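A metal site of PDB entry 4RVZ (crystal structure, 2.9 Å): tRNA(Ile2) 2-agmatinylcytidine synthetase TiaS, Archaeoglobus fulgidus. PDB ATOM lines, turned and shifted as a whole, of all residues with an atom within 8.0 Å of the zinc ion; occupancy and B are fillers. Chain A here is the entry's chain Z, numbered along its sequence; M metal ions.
The side-chain sulfur of Cys 355 sits close to the backbone NH of Arg 357, at 3.2 Å.
The side-chain amino group (NZ) of Lys 372 sits close to the side-chain sulfur (SG) of Cys 370 (3.5 Å).
The backbone NH of Cys 370 lies within hydrogen-bond range of the backbone carbonyl oxygen of Thr 375 (3.3 Å).
The side-chain sulfur (SG) of Cys 352 lies close to the backbone NH (N) of Ser 354 (3.4 Å).
The side-chain sulfur (SG) of Cys 352 lies close to the side-chain hydroxyl (OG1) of Thr 375, at 3.4 Å.
O of Arg 357 sits at hydrogen-bond distance from N of Cys 352 (2.8 Å).
SG of Cys 373 sits close to OG of Ser 354 (3.8 Å).
Of the 16 residues printed, 4 come within 4 Å of the zinc ion.
The nearest printed residue that does not touch the zinc ion is Lys 372 (4.1 Å).
The side-chain sulfur (SG) of Cys 355 binds the zinc ion.
The zinc ion is bound by SG of Cys 370.
The zinc ion is bound by the side-chain sulfur (SG) of Cys 352.
The side-chain sulfur (SG) of Cys 373 binds the zinc ion.
The zinc ion has four donor atoms within binding distance.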
ATOM      1  N   ILE A 351      -3.566 -14.242 -13.546  1.00  0.00           N
ATOM      2  CA  ILE A 351      -4.021 -15.291 -14.457  1.00  0.00           C
ATOM      3  C   ILE A 351      -2.841 -16.171 -14.873  1.00  0.00           C
ATOM      4  O   ILE A 351      -1.781 -15.671 -15.232  1.00  0.00           O
ATOM      5  CB  ILE A 351      -4.689 -14.717 -15.734  1.00  0.00           C
ATOM      6  CG1 ILE A 351      -6.149 -14.362 -15.458  1.00  0.00           C
ATOM      7  CG2 ILE A 351      -4.640 -15.711 -16.889  1.00  0.00           C
ATOM      8  CD1 ILE A 351      -6.333 -13.143 -14.605  1.00  0.00           C
ATOM      9  N   CYS A 352      -3.023 -17.490 -14.783  1.00  0.00           N
ATOM     10  CA  CYS A 352      -2.004 -18.431 -15.214  1.00  0.00           C
ATOM     11  C   CYS A 352      -1.727 -18.306 -16.709  1.00  0.00           C
ATOM     12  O   CYS A 352      -2.663 -18.317 -17.509  1.00  0.00           O
ATOM     13  CB  CYS A 352      -2.430 -19.864 -14.901  1.00  0.00           C
ATOM     14  SG  CYS A 352      -1.388 -21.102 -15.668  1.00  0.00           S
ATOM     15  N   PRO A 353      -0.442 -18.188 -17.092  1.00  0.00           N
ATOM     16  CA  PRO A 353      -0.018 -17.979 -18.484  1.00  0.00           C
ATOM     17  C   PRO A 353      -0.171 -19.198 -19.409  1.00  0.00           C
ATOM     18  O   PRO A 353       0.077 -19.067 -20.603  1.00  0.00           O
ATOM     19  CB  PRO A 353       1.459 -17.588 -18.341  1.00  0.00           C
ATOM     20  CG  PRO A 353       1.896 -18.191 -17.063  1.00  0.00           C
ATOM     21  CD  PRO A 353       0.694 -18.133 -16.151  1.00  0.00           C
ATOM     22  N   SER A 354      -0.556 -20.352 -18.874  1.00  0.00           N
ATOM     23  CA  SER A 354      -0.794 -21.523 -19.723  1.00  0.00           C
ATOM     24  C   SER A 354      -2.273 -21.878 -19.886  1.00  0.00           C
ATOM     25  O   SER A 354      -2.820 -21.813 -20.991  1.00  0.00           O
ATOM     26  CB  SER A 354      -0.045 -22.739 -19.180  1.00  0.00           C
ATOM     27  OG  SER A 354      -0.519 -23.910 -19.807  1.00  0.00           O
ATOM     28  N   CYS A 355      -2.913 -22.242 -18.771  1.00  0.00           N
ATOM     29  CA  CYS A 355      -4.298 -22.707 -18.775  1.00  0.00           C
ATOM     30  C   CYS A 355      -5.322 -21.559 -18.805  1.00  0.00           C
ATOM     31  O   CYS A 355      -6.445 -21.720 -19.292  1.00  0.00           O
ATOM     32  CB  CYS A 355      -4.551 -23.585 -17.543  1.00  0.00           C
ATOM     33  SG  CYS A 355      -4.504 -22.643 -16.017  1.00  0.00           S
ATOM     34  N   GLY A 356      -4.925 -20.406 -18.271  1.00  0.00           N
ATOM     35  CA  GLY A 356      -5.785 -19.249 -18.252  1.00  0.00           C
ATOM     36  C   GLY A 356      -6.490 -19.072 -16.926  1.00  0.00           C
ATOM     37  O   GLY A 356      -6.980 -17.983 -16.631  1.00  0.00           O
ATOM     38  N   ARG A 357      -6.538 -20.142 -16.123  1.00  0.00           N
ATOM     39  CA  ARG A 357      -7.265 -20.094 -14.855  1.00  0.00           C
ATOM     40  C   ARG A 357      -6.561 -19.176 -13.851  1.00  0.00           C
ATOM     41  O   ARG A 357      -5.418 -18.798 -14.057  1.00  0.00           O
ATOM     42  CB  ARG A 357      -7.492 -21.499 -14.271  1.00  0.00           C
ATOM     43  CG  ARG A 357      -6.454 -21.980 -13.271  1.00  0.00           C
ATOM     44  CD  ARG A 357      -7.038 -22.185 -11.880  1.00  0.00           C
ATOM     45  NE  ARG A 357      -8.288 -22.933 -11.878  1.00  0.00           N
ATOM     46  CZ  ARG A 357      -8.747 -23.632 -10.838  1.00  0.00           C
ATOM     47  NH1 ARG A 357      -8.038 -23.687  -9.715  1.00  0.00           N
ATOM     48  NH2 ARG A 357      -9.895 -24.276 -10.923  1.00  0.00           N
ATOM     49  N   ARG A 358      -7.266 -18.809 -12.785  1.00  0.00           N
ATOM     50  CA  ARG A 358      -6.736 -17.867 -11.819  1.00  0.00           C
ATOM     51  C   ARG A 358      -5.815 -18.595 -10.838  1.00  0.00           C
ATOM     52  O   ARG A 358      -6.181 -19.632 -10.293  1.00  0.00           O
ATOM     53  CB  ARG A 358      -7.877 -17.200 -11.046  1.00  0.00           C
ATOM     54  CG  ARG A 358      -7.499 -15.925 -10.326  1.00  0.00           C
ATOM     55  CD  ARG A 358      -8.458 -15.656  -9.166  1.00  0.00           C
ATOM     56  NE  ARG A 358      -8.268 -16.612  -8.087  1.00  0.00           N
ATOM     57  CZ  ARG A 358      -8.396 -16.330  -6.795  1.00  0.00           C
ATOM     58  NH1 ARG A 358      -8.188 -17.267  -5.879  1.00  0.00           N
ATOM     59  NH2 ARG A 358      -8.732 -15.098  -6.414  1.00  0.00           N
ATOM     60  N   MET A 359      -4.618 -18.043 -10.638  1.00  0.00           N
ATOM     61  CA  MET A 359      -3.690 -18.585  -9.656  1.00  0.00           C
ATOM     62  C   MET A 359      -4.270 -18.425  -8.261  1.00  0.00           C
ATOM     63  O   MET A 359      -4.927 -17.422  -7.953  1.00  0.00           O
ATOM     64  CB  MET A 359      -2.343 -17.860  -9.720  1.00  0.00           C
ATOM     65  CG  MET A 359      -1.552 -18.142 -10.981  1.00  0.00           C
ATOM     66  SD  MET A 359       0.113 -17.463 -10.949  1.00  0.00           S
ATOM     67  CE  MET A 359       0.661 -17.916 -12.584  1.00  0.00           C
ATOM     68  N   ARG A 369       0.514 -19.334  -7.568  1.00  0.00           N
ATOM     69  CA  ARG A 369       0.947 -20.335  -8.528  1.00  0.00           C
ATOM     70  C   ARG A 369      -0.209 -21.021  -9.192  1.00  0.00           C
ATOM     71  O   ARG A 369      -1.376 -20.743  -8.893  1.00  0.00           O
ATOM     72  CB  ARG A 369       1.852 -21.375  -7.855  1.00  0.00           C
ATOM     73  CG  ARG A 369       1.545 -21.631  -6.385  1.00  0.00           C
ATOM     74  CD  ARG A 369       0.261 -22.415  -6.163  1.00  0.00           C
ATOM     75  NE  ARG A 369       0.142 -22.829  -4.765  1.00  0.00           N
ATOM     76  CZ  ARG A 369      -0.805 -23.635  -4.289  1.00  0.00           C
ATOM     77  NH1 ARG A 369      -1.743 -24.124  -5.093  1.00  0.00           N
ATOM     78  NH2 ARG A 369      -0.812 -23.950  -2.998  1.00  0.00           N
ATOM     79  N   CYS A 370       0.106 -21.928 -10.096  1.00  0.00           N
ATOM     80  CA  CYS A 370      -0.889 -22.738 -10.779  1.00  0.00           C
ATOM     81  C   CYS A 370      -0.422 -24.165 -10.752  1.00  0.00           C
ATOM     82  O   CYS A 370       0.530 -24.525 -11.441  1.00  0.00           O
ATOM     83  CB  CYS A 370      -1.085 -22.274 -12.222  1.00  0.00           C
ATOM     84  SG  CYS A 370      -2.175 -23.351 -13.189  1.00  0.00           S
ATOM     85  N   LYS A 371      -1.096 -24.992  -9.965  1.00  0.00           N
ATOM     86  CA  LYS A 371      -0.690 -26.381  -9.789  1.00  0.00           C
ATOM     87  C   LYS A 371      -0.871 -27.234 -11.040  1.00  0.00           C
ATOM     88  O   LYS A 371      -0.127 -28.187 -11.253  1.00  0.00           O
ATOM     89  CB  LYS A 371      -1.399 -27.011  -8.575  1.00  0.00           C
ATOM     90  CG  LYS A 371      -0.784 -26.618  -7.237  1.00  0.00           C
ATOM     91  CD  LYS A 371      -1.193 -27.587  -6.127  1.00  0.00           C
ATOM     92  CE  LYS A 371      -0.399 -27.349  -4.850  1.00  0.00           C
ATOM     93  NZ  LYS A 371      -0.731 -28.336  -3.782  1.00  0.00           N
ATOM     94  N   LYS A 372      -1.837 -26.875 -11.887  1.00  0.00           N
ATOM     95  CA  LYS A 372      -2.068 -27.630 -13.120  1.00  0.00           C
ATOM     96  C   LYS A 372      -0.948 -27.411 -14.144  1.00  0.00           C
ATOM     97  O   LYS A 372      -0.952 -27.986 -15.233  1.00  0.00           O
ATOM     98  CB  LYS A 372      -3.448 -27.315 -13.731  1.00  0.00           C
ATOM     99  CG  LYS A 372      -4.187 -26.135 -13.103  1.00  0.00           C
ATOM    100  CD  LYS A 372      -4.967 -26.538 -11.843  1.00  0.00           C
ATOM    101  CE  LYS A 372      -4.559 -25.692 -10.646  1.00  0.00           C
ATOM    102  NZ  LYS A 372      -4.651 -24.231 -10.903  1.00  0.00           N
ATOM    103  N   CYS A 373       0.015 -26.562 -13.771  1.00  0.00           N
ATOM    104  CA  CYS A 373       1.256 -26.405 -14.505  1.00  0.00           C
ATOM    105  C   CYS A 373       2.339 -26.297 -13.440  1.00  0.00           C
ATOM    106  O   CYS A 373       2.123 -26.667 -12.287  1.00  0.00           O
ATOM    107  CB  CYS A 373       1.228 -25.141 -15.346  1.00  0.00           C
ATOM    108  SG  CYS A 373      -0.347 -24.851 -16.177  1.00  0.00           S
ATOM    109  N   ARG A 374       3.508 -25.807 -13.813  1.00  0.00           N
ATOM    110  CA  ARG A 374       4.512 -25.462 -12.818  1.00  0.00           C
ATOM    111  C   ARG A 374       4.772 -23.971 -12.898  1.00  0.00           C
ATOM    112  O   ARG A 374       5.923 -23.524 -12.812  1.00  0.00           O
ATOM    113  CB  ARG A 374       5.806 -26.242 -12.999  1.00  0.00           C
ATOM    114  CG  ARG A 374       5.893 -27.536 -12.195  1.00  0.00           C
ATOM    115  CD  ARG A 374       7.333 -28.031 -12.068  1.00  0.00           C
ATOM    116  NE  ARG A 374       8.161 -27.101 -11.305  1.00  0.00           N
ATOM    117  CZ  ARG A 374       8.491 -27.262 -10.025  1.00  0.00           C
ATOM    118  NH1 ARG A 374       8.073 -28.320  -9.358  1.00  0.00           N
ATOM    119  NH2 ARG A 374       9.249 -26.356  -9.416  1.00  0.00           N
ATOM    120  N   THR A 375       3.705 -23.206 -13.070  1.00  0.00           N
ATOM    121  CA  THR A 375       3.838 -21.773 -13.271  1.00  0.00           C
ATOM    122  C   THR A 375       3.681 -20.965 -11.986  1.00  0.00           C
ATOM    123  O   THR A 375       3.206 -21.476 -10.976  1.00  0.00           O
ATOM    124  CB  THR A 375       2.883 -21.261 -14.358  1.00  0.00           C
ATOM    125  OG1 THR A 375       1.519 -21.531 -13.990  1.00  0.00           O
ATOM    126  CG2 THR A 375       3.177 -21.967 -15.669  1.00  0.00           C
HETATM  127 ZN    ZN M   1      -2.324 -23.336 -15.530  1.00  0.00          ZN
